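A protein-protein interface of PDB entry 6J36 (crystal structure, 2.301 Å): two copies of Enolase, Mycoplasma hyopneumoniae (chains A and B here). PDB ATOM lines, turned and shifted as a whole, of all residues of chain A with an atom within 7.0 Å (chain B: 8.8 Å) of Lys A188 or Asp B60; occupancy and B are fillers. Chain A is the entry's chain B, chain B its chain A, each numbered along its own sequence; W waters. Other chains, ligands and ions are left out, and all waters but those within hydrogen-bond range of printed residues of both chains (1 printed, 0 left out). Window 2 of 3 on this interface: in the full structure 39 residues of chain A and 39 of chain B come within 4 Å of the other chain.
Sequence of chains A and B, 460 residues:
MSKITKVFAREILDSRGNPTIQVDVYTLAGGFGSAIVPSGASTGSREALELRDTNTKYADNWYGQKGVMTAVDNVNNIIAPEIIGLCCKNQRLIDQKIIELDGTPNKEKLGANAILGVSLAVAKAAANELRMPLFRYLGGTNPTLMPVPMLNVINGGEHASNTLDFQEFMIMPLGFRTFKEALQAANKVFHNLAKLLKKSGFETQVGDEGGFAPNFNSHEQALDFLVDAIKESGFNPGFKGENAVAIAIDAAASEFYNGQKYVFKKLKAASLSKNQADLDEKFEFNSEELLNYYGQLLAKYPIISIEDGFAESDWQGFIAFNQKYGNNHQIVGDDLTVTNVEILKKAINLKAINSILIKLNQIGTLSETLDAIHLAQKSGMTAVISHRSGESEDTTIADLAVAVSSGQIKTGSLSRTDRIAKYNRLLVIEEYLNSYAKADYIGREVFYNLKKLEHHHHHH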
ATOM      1  N   ALA A 182       5.090 -18.247  23.596  1.00  0.00           N
ATOM      2  CA  ALA A 182       4.407 -19.361  22.947  1.00  0.00           C
ATOM      3  C   ALA A 182       5.257 -19.929  21.819  1.00  0.00           C
ATOM      4  O   ALA A 182       5.354 -21.151  21.655  1.00  0.00           O
ATOM      5  CB  ALA A 182       3.041 -18.908  22.438  1.00  0.00           C
ATOM      6  N   LEU A 183       5.915 -19.057  21.057  1.00  0.00           N
ATOM      7  CA  LEU A 183       6.764 -19.525  19.973  1.00  0.00           C
ATOM      8  C   LEU A 183       8.011 -20.215  20.513  1.00  0.00           C
ATOM      9  O   LEU A 183       8.449 -21.238  19.969  1.00  0.00           O
ATOM     10  CB  LEU A 183       7.121 -18.353  19.064  1.00  0.00           C
ATOM     11  CG  LEU A 183       7.876 -18.693  17.775  1.00  0.00           C
ATOM     12  CD1 LEU A 183       7.091 -19.665  16.880  1.00  0.00           C
ATOM     13  CD2 LEU A 183       8.252 -17.416  17.022  1.00  0.00           C
ATOM     14  N   GLN A 184       8.586 -19.674  21.593  1.00  0.00           N
ATOM     15  CA  GLN A 184       9.709 -20.324  22.264  1.00  0.00           C
ATOM     16  C   GLN A 184       9.336 -21.728  22.727  1.00  0.00           C
ATOM     17  O   GLN A 184      10.094 -22.682  22.516  1.00  0.00           O
ATOM     18  CB  GLN A 184      10.188 -19.457  23.437  1.00  0.00           C
ATOM     19  CG  GLN A 184      10.974 -18.226  22.933  1.00  0.00           C
ATOM     20  CD  GLN A 184      11.227 -17.158  23.972  1.00  0.00           C
ATOM     21  OE1 GLN A 184      10.664 -17.182  25.060  1.00  0.00           O
ATOM     22  NE2 GLN A 184      12.090 -16.206  23.635  1.00  0.00           N
ATOM     23  N   ALA A 185       8.152 -21.883  23.328  1.00  0.00           N
ATOM     24  CA  ALA A 185       7.700 -23.211  23.732  1.00  0.00           C
ATOM     25  C   ALA A 185       7.607 -24.143  22.533  1.00  0.00           C
ATOM     26  O   ALA A 185       8.075 -25.289  22.588  1.00  0.00           O
ATOM     27  CB  ALA A 185       6.344 -23.115  24.439  1.00  0.00           C
ATOM     28  N   ALA A 186       6.989 -23.668  21.437  1.00  0.00           N
ATOM     29  CA  ALA A 186       6.928 -24.454  20.204  1.00  0.00           C
ATOM     30  C   ALA A 186       8.321 -24.817  19.702  1.00  0.00           C
ATOM     31  O   ALA A 186       8.542 -25.930  19.210  1.00  0.00           O
ATOM     32  CB  ALA A 186       6.157 -23.689  19.120  1.00  0.00           C
ATOM     33  N   ASN A 187       9.272 -23.886  19.802  1.00  0.00           N
ATOM     34  CA  ASN A 187      10.638 -24.199  19.388  1.00  0.00           C
ATOM     35  C   ASN A 187      11.227 -25.299  20.255  1.00  0.00           C
ATOM     36  O   ASN A 187      11.937 -26.181  19.753  1.00  0.00           O
ATOM     37  CB  ASN A 187      11.493 -22.921  19.401  1.00  0.00           C
ATOM     38  CG  ASN A 187      12.992 -23.185  19.601  1.00  0.00           C
ATOM     39  OD1 ASN A 187      13.434 -23.450  20.703  1.00  0.00           O
ATOM     40  ND2 ASN A 187      13.774 -23.052  18.540  1.00  0.00           N
ATOM     41  N   LYS A 188      10.902 -25.298  21.549  1.00  0.00           N
ATOM     42  CA  LYS A 188      11.425 -26.337  22.428  1.00  0.00           C
ATOM     43  C   LYS A 188      10.776 -27.688  22.143  1.00  0.00           C
ATOM     44  O   LYS A 188      11.467 -28.711  22.119  1.00  0.00           O
ATOM     45  CB  LYS A 188      11.260 -25.913  23.901  1.00  0.00           C
ATOM     46  CG  LYS A 188      12.351 -24.930  24.338  1.00  0.00           C
ATOM     47  CD  LYS A 188      12.011 -24.158  25.604  1.00  0.00           C
ATOM     48  CE  LYS A 188      13.109 -23.148  25.913  1.00  0.00           C
ATOM     49  NZ  LYS A 188      13.017 -22.538  27.282  1.00  0.00           N
ATOM     50  N   VAL A 189       9.458 -27.724  21.914  1.00  0.00           N
ATOM     51  CA  VAL A 189       8.802 -29.004  21.617  1.00  0.00           C
ATOM     52  C   VAL A 189       9.309 -29.574  20.296  1.00  0.00           C
ATOM     53  O   VAL A 189       9.576 -30.779  20.183  1.00  0.00           O
ATOM     54  CB  VAL A 189       7.268 -28.848  21.618  1.00  0.00           C
ATOM     55  CG1 VAL A 189       6.575 -30.153  21.154  1.00  0.00           C
ATOM     56  CG2 VAL A 189       6.795 -28.463  23.001  1.00  0.00           C
ATOM     57  N   PHE A 190       9.484 -28.711  19.290  1.00  0.00           N
ATOM     58  CA  PHE A 190       9.894 -29.171  17.964  1.00  0.00           C
ATOM     59  C   PHE A 190      11.283 -29.796  18.003  1.00  0.00           C
ATOM     60  O   PHE A 190      11.502 -30.892  17.473  1.00  0.00           O
ATOM     61  CB  PHE A 190       9.831 -27.995  16.983  1.00  0.00           C
ATOM     62  CG  PHE A 190      10.489 -28.246  15.635  1.00  0.00           C
ATOM     63  CD1 PHE A 190       9.761 -28.792  14.578  1.00  0.00           C
ATOM     64  CD2 PHE A 190      11.815 -27.872  15.409  1.00  0.00           C
ATOM     65  CE1 PHE A 190      10.348 -28.987  13.328  1.00  0.00           C
ATOM     66  CE2 PHE A 190      12.411 -28.078  14.174  1.00  0.00           C
ATOM     67  CZ  PHE A 190      11.676 -28.636  13.125  1.00  0.00           C
ATOM     68  N   HIS A 191      12.233 -29.130  18.657  1.00  0.00           N
ATOM     69  CA  HIS A 191      13.598 -29.648  18.678  1.00  0.00           C
ATOM     70  C   HIS A 191      13.734 -30.866  19.594  1.00  0.00           C
ATOM     71  O   HIS A 191      14.480 -31.796  19.282  1.00  0.00           O
ATOM     72  CB  HIS A 191      14.554 -28.538  19.093  1.00  0.00           C
ATOM     73  CG  HIS A 191      14.736 -27.498  18.039  1.00  0.00           C
ATOM     74  ND1 HIS A 191      15.245 -27.788  16.789  1.00  0.00           N
ATOM     75  CD2 HIS A 191      14.468 -26.171  18.040  1.00  0.00           C
ATOM     76  CE1 HIS A 191      15.287 -26.683  16.066  1.00  0.00           C
ATOM     77  NE2 HIS A 191      14.823 -25.686  16.801  1.00  0.00           N
ATOM     78  N   ASN A 192      13.031 -30.868  20.730  1.00  0.00           N
ATOM     79  CA  ASN A 192      12.977 -32.052  21.581  1.00  0.00           C
ATOM     80  C   ASN A 192      12.287 -33.209  20.878  1.00  0.00           C
ATOM     81  O   ASN A 192      12.683 -34.365  21.051  1.00  0.00           O
ATOM     82  CB  ASN A 192      12.245 -31.736  22.882  1.00  0.00           C
ATOM     83  CG  ASN A 192      13.176 -31.238  23.960  1.00  0.00           C
ATOM     84  OD1 ASN A 192      14.140 -31.903  24.304  1.00  0.00           O
ATOM     85  ND2 ASN A 192      12.904 -30.056  24.480  1.00  0.00           N
ATOM     86  N   LEU A 193      11.224 -32.921  20.115  1.00  0.00           N
ATOM     87  CA  LEU A 193      10.600 -33.960  19.298  1.00  0.00           C
ATOM     88  C   LEU A 193      11.620 -34.586  18.354  1.00  0.00           C
ATOM     89  O   LEU A 193      11.750 -35.809  18.299  1.00  0.00           O
ATOM     90  CB  LEU A 193       9.408 -33.395  18.511  1.00  0.00           C
ATOM     91  CG  LEU A 193       8.674 -34.385  17.591  1.00  0.00           C
ATOM     92  CD1 LEU A 193       8.160 -35.607  18.368  1.00  0.00           C
ATOM     93  CD2 LEU A 193       7.519 -33.721  16.866  1.00  0.00           C
ATOM     94  N   ALA A 194      12.383 -33.754  17.632  1.00  0.00           N
ATOM     95  CA  ALA A 194      13.405 -34.280  16.729  1.00  0.00           C
ATOM     96  C   ALA A 194      14.440 -35.113  17.480  1.00  0.00           C
ATOM     97  O   ALA A 194      14.845 -36.183  17.010  1.00  0.00           O
ATOM     98  CB  ALA A 194      14.088 -33.144  15.965  1.00  0.00           C
ATOM     99  N   ALA A 229       6.999 -35.890  24.084  1.00  0.00           N
ATOM    100  CA  ALA A 229       7.891 -34.795  23.712  1.00  0.00           C
ATOM    101  C   ALA A 229       7.484 -33.489  24.388  1.00  0.00           C
ATOM    102  O   ALA A 229       8.344 -32.697  24.792  1.00  0.00           O
ATOM    103  CB  ALA A 229       7.919 -34.628  22.192  1.00  0.00           C
ATOM    104  N   GLU A 232       8.786 -33.860  27.873  1.00  0.00           N
ATOM    105  CA  GLU A 232      10.243 -33.736  27.886  1.00  0.00           C
ATOM    106  C   GLU A 232      10.701 -32.279  27.816  1.00  0.00           C
ATOM    107  O   GLU A 232      11.722 -31.916  28.414  1.00  0.00           O
ATOM    108  CB  GLU A 232      10.837 -34.527  26.718  1.00  0.00           C
ATOM    109  CG  GLU A 232      12.170 -35.188  27.022  1.00  0.00           C
ATOM    110  CD  GLU A 232      12.045 -36.213  28.125  1.00  0.00           C
ATOM    111  OE1 GLU A 232      12.868 -36.161  29.065  1.00  0.00           O
ATOM    112  OE2 GLU A 232      11.111 -37.054  28.055  1.00  0.00           O
ATOM    113  N   SER A 233       9.984 -31.436  27.066  1.00  0.00           N
ATOM    114  CA  SER A 233      10.340 -30.025  26.906  1.00  0.00           C
ATOM    115  C   SER A 233      10.011 -29.175  28.125  1.00  0.00           C
ATOM    116  O   SER A 233      10.352 -27.991  28.130  1.00  0.00           O
ATOM    117  CB  SER A 233       9.623 -29.408  25.693  1.00  0.00           C
ATOM    118  OG  SER A 233       9.560 -30.304  24.606  1.00  0.00           O
ATOM    119  N   GLY A 234       9.341 -29.731  29.134  1.00  0.00           N
ATOM    120  CA  GLY A 234       8.977 -28.994  30.327  1.00  0.00           C
ATOM    121  C   GLY A 234       7.558 -28.452  30.375  1.00  0.00           C
ATOM    122  O   GLY A 234       7.276 -27.597  31.228  1.00  0.00           O
ATOM    123  N   PHE A 235       6.651 -28.929  29.513  1.00  0.00           N
ATOM    124  CA  PHE A 235       5.302 -28.380  29.420  1.00  0.00           C
ATOM    125  C   PHE A 235       4.255 -29.441  29.757  1.00  0.00           C
ATOM    126  O   PHE A 235       4.562 -30.618  29.936  1.00  0.00           O
ATOM    127  CB  PHE A 235       5.061 -27.769  28.024  1.00  0.00           C
ATOM    128  CG  PHE A 235       6.147 -26.809  27.608  1.00  0.00           C
ATOM    129  CD1 PHE A 235       6.447 -25.700  28.399  1.00  0.00           C
ATOM    130  CD2 PHE A 235       6.912 -27.045  26.478  1.00  0.00           C
ATOM    131  CE1 PHE A 235       7.461 -24.814  28.040  1.00  0.00           C
ATOM    132  CE2 PHE A 235       7.947 -26.170  26.126  1.00  0.00           C
ATOM    133  CZ  PHE A 235       8.217 -25.054  26.902  1.00  0.00           C
ATOM    134  N   LEU A 414       8.176 -25.750  12.365  1.00  0.00           N
ATOM    135  CA  LEU A 414       9.213 -24.759  12.659  1.00  0.00           C
ATOM    136  C   LEU A 414      10.490 -24.953  11.843  1.00  0.00           C
ATOM    137  O   LEU A 414      11.601 -24.755  12.359  1.00  0.00           O
ATOM    138  CB  LEU A 414       9.536 -24.765  14.145  1.00  0.00           C
ATOM    139  CG  LEU A 414       8.812 -23.760  15.037  1.00  0.00           C
ATOM    140  CD1 LEU A 414       9.681 -23.490  16.197  1.00  0.00           C
ATOM    141  CD2 LEU A 414       8.469 -22.458  14.326  1.00  0.00           C
ATOM    142  N   LEU B  13      13.845 -16.165  13.594  1.00  0.00           N
ATOM    143  CA  LEU B  13      14.219 -17.566  13.426  1.00  0.00           C
ATOM    144  C   LEU B  13      14.751 -17.824  12.022  1.00  0.00           C
ATOM    145  O   LEU B  13      14.336 -17.174  11.057  1.00  0.00           O
ATOM    146  CB  LEU B  13      13.038 -18.497  13.692  1.00  0.00           C
ATOM    147  CG  LEU B  13      12.516 -18.549  15.128  1.00  0.00           C
ATOM    148  CD1 LEU B  13      11.291 -19.433  15.184  1.00  0.00           C
ATOM    149  CD2 LEU B  13      13.607 -19.030  16.138  1.00  0.00           C
ATOM    150  N   GLY B  17      14.713 -23.348  12.264  1.00  0.00           N
ATOM    151  CA  GLY B  17      14.047 -23.111  13.526  1.00  0.00           C
ATOM    152  C   GLY B  17      14.953 -22.719  14.668  1.00  0.00           C
ATOM    153  O   GLY B  17      14.606 -22.958  15.828  1.00  0.00           O
ATOM    154  N   ASN B  18      16.101 -22.116  14.386  1.00  0.00           N
ATOM    155  CA  ASN B  18      16.983 -21.618  15.433  1.00  0.00           C
ATOM    156  C   ASN B  18      17.093 -20.106  15.331  1.00  0.00           C
ATOM    157  O   ASN B  18      16.978 -19.555  14.238  1.00  0.00           O
ATOM    158  CB  ASN B  18      18.384 -22.236  15.334  1.00  0.00           C
ATOM    159  CG  ASN B  18      18.376 -23.744  15.623  1.00  0.00           C
ATOM    160  OD1 ASN B  18      17.856 -24.186  16.654  1.00  0.00           O
ATOM    161  ND2 ASN B  18      18.933 -24.530  14.711  1.00  0.00           N
ATOM    162  N   ASP B  53      23.754 -17.158  22.866  1.00  0.00           N
ATOM    163  CA  ASP B  53      23.399 -16.662  24.184  1.00  0.00           C
ATOM    164  C   ASP B  53      23.873 -17.579  25.321  1.00  0.00           C
ATOM    165  O   ASP B  53      23.394 -17.445  26.451  1.00  0.00           O
ATOM    166  CB  ASP B  53      21.888 -16.431  24.247  1.00  0.00           C
ATOM    167  CG  ASP B  53      21.465 -15.166  23.507  1.00  0.00           C
ATOM    168  OD1 ASP B  53      22.344 -14.317  23.239  1.00  0.00           O
ATOM    169  OD2 ASP B  53      20.263 -15.015  23.181  1.00  0.00           O
ATOM    170  N   THR B  54      24.796 -18.497  25.041  1.00  0.00           N
ATOM    171  CA  THR B  54      25.362 -19.370  26.066  1.00  0.00           C
ATOM    172  C   THR B  54      25.850 -18.565  27.261  1.00  0.00           C
ATOM    173  O   THR B  54      26.536 -17.552  27.090  1.00  0.00           O
ATOM    174  CB  THR B  54      26.544 -20.150  25.488  1.00  0.00           C
ATOM    175  OG1 THR B  54      26.289 -20.490  24.116  1.00  0.00           O
ATOM    176  CG2 THR B  54      26.799 -21.413  26.309  1.00  0.00           C
ATOM    177  N   ASN B  55      25.494 -19.020  28.466  1.00  0.00           N
ATOM    178  CA  ASN B  55      25.954 -18.406  29.721  1.00  0.00           C
ATOM    179  C   ASN B  55      25.637 -16.921  29.784  1.00  0.00           C
ATOM    180  O   ASN B  55      26.494 -16.089  30.084  1.00  0.00           O
ATOM    181  CB  ASN B  55      27.450 -18.632  29.936  1.00  0.00           C
ATOM    182  CG  ASN B  55      27.764 -20.077  30.188  1.00  0.00           C
ATOM    183  OD1 ASN B  55      28.505 -20.697  29.435  1.00  0.00           O
ATOM    184  ND2 ASN B  55      27.153 -20.644  31.228  1.00  0.00           N
ATOM    185  N   THR B  56      24.400 -16.588  29.438  1.00  0.00           N
ATOM    186  CA  THR B  56      23.854 -15.252  29.588  1.00  0.00           C
ATOM    187  C   THR B  56      22.473 -15.409  30.189  1.00  0.00           C
ATOM    188  O   THR B  56      21.918 -16.511  30.221  1.00  0.00           O
ATOM    189  CB  THR B  56      23.728 -14.490  28.254  1.00  0.00           C
ATOM    190  OG1 THR B  56      22.597 -15.003  27.539  1.00  0.00           O
ATOM    191  CG2 THR B  56      24.985 -14.615  27.394  1.00  0.00           C
ATOM    192  N   LYS B  57      21.904 -14.288  30.638  1.00  0.00           N
ATOM    193  CA  LYS B  57      20.528 -14.282  31.118  1.00  0.00           C
ATOM    194  C   LYS B  57      19.533 -14.707  30.046  1.00  0.00           C
ATOM    195  O   LYS B  57      18.357 -14.939  30.365  1.00  0.00           O
ATOM    196  CB  LYS B  57      20.163 -12.892  31.628  1.00  0.00           C
ATOM    197  CG  LYS B  57      20.247 -11.803  30.561  1.00  0.00           C
ATOM    198  CD  LYS B  57      19.646 -10.489  31.068  1.00  0.00           C
ATOM    199  CE  LYS B  57      19.798  -9.375  30.042  1.00  0.00           C
ATOM    200  NZ  LYS B  57      19.731  -8.038  30.682  1.00  0.00           N
ATOM    201  N   TYR B  58      19.971 -14.809  28.793  1.00  0.00           N
ATOM    202  CA  TYR B  58      19.109 -15.184  27.683  1.00  0.00           C
ATOM    203  C   TYR B  58      19.153 -16.674  27.368  1.00  0.00           C
ATOM    204  O   TYR B  58      18.376 -17.131  26.519  1.00  0.00           O
ATOM    205  CB  TYR B  58      19.515 -14.416  26.421  1.00  0.00           C
ATOM    206  CG  TYR B  58      19.391 -12.916  26.509  1.00  0.00           C
ATOM    207  CD1 TYR B  58      18.171 -12.308  26.792  1.00  0.00           C
ATOM    208  CD2 TYR B  58      20.497 -12.104  26.286  1.00  0.00           C
ATOM    209  CE1 TYR B  58      18.065 -10.929  26.843  1.00  0.00           C
ATOM    210  CE2 TYR B  58      20.403 -10.741  26.336  1.00  0.00           C
ATOM    211  CZ  TYR B  58      19.193 -10.153  26.618  1.00  0.00           C
ATOM    212  OH  TYR B  58      19.114  -8.774  26.658  1.00  0.00           O
ATOM    213  N   ALA B  59      20.037 -17.434  28.027  1.00  0.00           N
ATOM    214  CA  ALA B  59      20.332 -18.797  27.593  1.00  0.00           C
ATOM    215  C   ALA B  59      19.079 -19.660  27.529  1.00  0.00           C
ATOM    216  O   ALA B  59      18.946 -20.518  26.648  1.00  0.00           O
ATOM    217  CB  ALA B  59      21.378 -19.421  28.524  1.00  0.00           C
ATOM    218  N   ASP B  60      18.136 -19.432  28.430  1.00  0.00           N
ATOM    219  CA  ASP B  60      16.946 -20.268  28.498  1.00  0.00           C
ATOM    220  C   ASP B  60      15.858 -19.879  27.496  1.00  0.00           C
ATOM    221  O   ASP B  60      14.822 -20.546  27.466  1.00  0.00           O
ATOM    222  CB  ASP B  60      16.381 -20.226  29.924  1.00  0.00           C
ATOM    223  CG  ASP B  60      15.795 -21.552  30.352  1.00  0.00           C
ATOM    224  OD1 ASP B  60      16.315 -22.595  29.903  1.00  0.00           O
ATOM    225  OD2 ASP B  60      14.812 -21.560  31.132  1.00  0.00           O
ATOM    226  N   ASN B  61      16.059 -18.838  26.673  1.00  0.00           N
ATOM    227  CA  ASN B  61      14.994 -18.373  25.773  1.00  0.00           C
ATOM    228  C   ASN B  61      14.605 -19.429  24.743  1.00  0.00           C
ATOM    229  O   ASN B  61      13.416 -19.637  24.482  1.00  0.00           O
ATOM    230  CB  ASN B  61      15.426 -17.098  25.039  1.00  0.00           C
ATOM    231  CG  ASN B  61      15.295 -15.848  25.895  1.00  0.00           C
ATOM    232  OD1 ASN B  61      14.633 -15.854  26.919  1.00  0.00           O
ATOM    233  ND2 ASN B  61      15.919 -14.766  25.453  1.00  0.00           N
ATOM    234  N   TRP B  62      15.584 -20.089  24.133  1.00  0.00           N
ATOM    235  CA  TRP B  62      15.345 -20.994  23.009  1.00  0.00           C
ATOM    236  C   TRP B  62      16.105 -22.295  23.214  1.00  0.00           C
ATOM    237  O   TRP B  62      17.122 -22.330  23.909  1.00  0.00           O
ATOM    238  CB  TRP B  62      15.798 -20.375  21.682  1.00  0.00           C
ATOM    239  CG  TRP B  62      15.194 -19.045  21.384  1.00  0.00           C
ATOM    240  CD1 TRP B  62      15.709 -17.807  21.693  1.00  0.00           C
ATOM    241  CD2 TRP B  62      13.972 -18.808  20.686  1.00  0.00           C
ATOM    242  NE1 TRP B  62      14.869 -16.821  21.239  1.00  0.00           N
ATOM    243  CE2 TRP B  62      13.792 -17.410  20.621  1.00  0.00           C
ATOM    244  CE3 TRP B  62      13.002 -19.646  20.116  1.00  0.00           C
ATOM    245  CZ2 TRP B  62      12.689 -16.830  19.998  1.00  0.00           C
ATOM    246  CZ3 TRP B  62      11.902 -19.069  19.501  1.00  0.00           C
ATOM    247  CH2 TRP B  62      11.753 -17.674  19.448  1.00  0.00           C
ATOM    248  N   TYR B  63      15.639 -23.350  22.543  1.00  0.00           N
ATOM    249  CA  TYR B  63      16.290 -24.655  22.631  1.00  0.00           C
ATOM    250  C   TYR B  63      17.787 -24.561  22.356  1.00  0.00           C
ATOM    251  O   TYR B  63      18.240 -23.773  21.519  1.00  0.00           O
ATOM    252  CB  TYR B  63      15.672 -25.630  21.634  1.00  0.00           C
ATOM    253  CG  TYR B  63      16.272 -27.021  21.698  1.00  0.00           C
ATOM    254  CD1 TYR B  63      15.786 -27.975  22.599  1.00  0.00           C
ATOM    255  CD2 TYR B  63      17.330 -27.375  20.874  1.00  0.00           C
ATOM    256  CE1 TYR B  63      16.331 -29.238  22.661  1.00  0.00           C
ATOM    257  CE2 TYR B  63      17.886 -28.628  20.933  1.00  0.00           C
ATOM    258  CZ  TYR B  63      17.383 -29.558  21.815  1.00  0.00           C
ATOM    259  OH  TYR B  63      17.955 -30.807  21.831  1.00  0.00           O
ATOM    260  N   GLY B  64      18.555 -25.406  23.047  1.00  0.00           N
ATOM    261  CA  GLY B  64      19.990 -25.480  22.836  1.00  0.00           C
ATOM    262  C   GLY B  64      20.764 -24.241  23.225  1.00  0.00           C
ATOM    263  O   GLY B  64      21.920 -24.114  22.824  1.00  0.00           O
ATOM    264  N   GLN B  65      20.166 -23.323  23.985  1.00  0.00           N
ATOM    265  CA  GLN B  65      20.780 -22.024  24.289  1.00  0.00           C
ATOM    266  C   GLN B  65      21.223 -21.294  23.018  1.00  0.00           C
ATOM    267  O   GLN B  65      22.317 -20.737  22.949  1.00  0.00           O
ATOM    268  CB  GLN B  65      21.974 -22.180  25.248  1.00  0.00           C
ATOM    269  CG  GLN B  65      21.656 -22.822  26.576  1.00  0.00           C
ATOM    270  CD  GLN B  65      21.662 -24.335  26.491  1.00  0.00           C
ATOM    271  OE1 GLN B  65      20.636 -24.988  26.716  1.00  0.00           O
ATOM    272  NE2 GLN B  65      22.821 -24.906  26.150  1.00  0.00           N
ATOM    273  N   LYS B  66      20.378 -21.289  21.991  1.00  0.00           N
ATOM    274  CA  LYS B  66      20.808 -20.799  20.691  1.00  0.00           C
ATOM    275  C   LYS B  66      20.359 -19.373  20.391  1.00  0.00           C
ATOM    276  O   LYS B  66      20.507 -18.919  19.255  1.00  0.00           O
ATOM    277  CB  LYS B  66      20.317 -21.747  19.597  1.00  0.00           C
ATOM    278  CG  LYS B  66      21.083 -23.053  19.518  1.00  0.00           C
ATOM    279  CD  LYS B  66      20.760 -23.761  18.213  1.00  0.00           C
ATOM    280  CE  LYS B  66      21.745 -24.886  17.904  1.00  0.00           C
ATOM    281  NZ  LYS B  66      21.139 -26.245  18.087  1.00  0.00           N
ATOM    282  N   GLY B  67      19.804 -18.660  21.363  1.00  0.00           N
ATOM    283  CA  GLY B  67      19.379 -17.295  21.117  1.00  0.00           C
ATOM    284  C   GLY B  67      20.527 -16.413  20.670  1.00  0.00           C
ATOM    285  O   GLY B  67      21.703 -16.757  20.815  1.00  0.00           O
HETATM  286  O   HOH W   1      16.566 -23.012  19.078  1.00  0.00           O
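O of Gly B17 lies within hydrogen-bond range of ND2 of Asn A187 (2.8 Å). A ring nitrogen (NE2) of His A191 sits at hydrogen-bond distance from the backbone carbonyl oxygen of Gly B17, 2.9 Å away. The backbone NH of Gly B17 sits close to the backbone carbonyl oxygen of Leu A414, 3.4 Å away. A ring nitrogen (NE2) of His A191 lies within hydrogen-bond range of the side-chain amide oxygen (OD1) of Asn B18 (3.4 Å). The side-chain amino group (NZ) of Lys A188 is in hydrogen-bond range of the backbone carbonyl oxygen (O) of Asp B60 (2.7 Å). The side-chain amide oxygen of Asn A187 is in hydrogen-bond range of the backbone NH of Tyr B63, 2.9 Å away.
The side-chain amide nitrogen (ND2) of Asn A187 sits close to a ring nitrogen (NE2) of His A191, 3.3 Å away. The backbone carbonyl oxygen of Lys A188 lies within hydrogen-bond range of the side-chain amide nitrogen of Asn A192, at 3.1 Å. OG of Ser A233 sits at hydrogen-bond distance from ND2 of Asn A192, 3.4 Å away.
Among the printed residues, merely in contact across the chains: Gln A184 with Asn B61, His A191 with Tyr B63, Asn A187 with Trp B62, Gln A184 with Trp B62, Lys A188 with Asn B61 and Asn A192 with Tyr B63.
Of the printed residues of chain B, Gln A184 touches Asn B61 (3.2 Å) and Trp B62 (3.6 Å). Lys A188 touches two residues of chain B. Of the printed residues of chain B, His A191 touches Gly B17, Asn B18 and Tyr B63. Printed residues of chain A within 4 Å of Gly B17: Asn A187 (2.8 Å), His A191 (2.9 Å) and Leu A414 (3.2 Å). Of the printed residues of chain A, Asn B18 touches His A191 (3.4 Å). Asp B60 touches one residue of chain A. The nearest residue of chain B that does not touch Lys A188 is Tyr B63 (4.1 Å). The nearest printed residue of chain A that does not touch Trp B62 is Leu A183 (4.1 Å).
Printed residues of chain B that touch a printed residue of chain A: Gly B17, Asn B18, Asp B60, Asn B61, Trp B62 and Tyr B63. Of the 19 printed residues of chain A, 6 touch a printed residue of chain B. Printed residues of chain A that touch a printed residue of chain B: Gln A184, Asn A187, Lys A188, His A191, Asn A192 and Leu A414. Hydrophobic or aromatic side chains of chain A within 4 Å of the printed part of chain B: His A191. Among the printed residues, no Asp or Glu carboxylate lies within 4 Å of a Lys or Arg side-chain nitrogen of the other chain.
No position is printed for both chains.
Water W1 lies within hydrogen-bond range of the side-chain amide nitrogen (ND2) of Asn A187, the side-chain amide oxygen (OD1) of Asn B18 and the backbone carbonyl oxygen (O) of Tyr B63.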
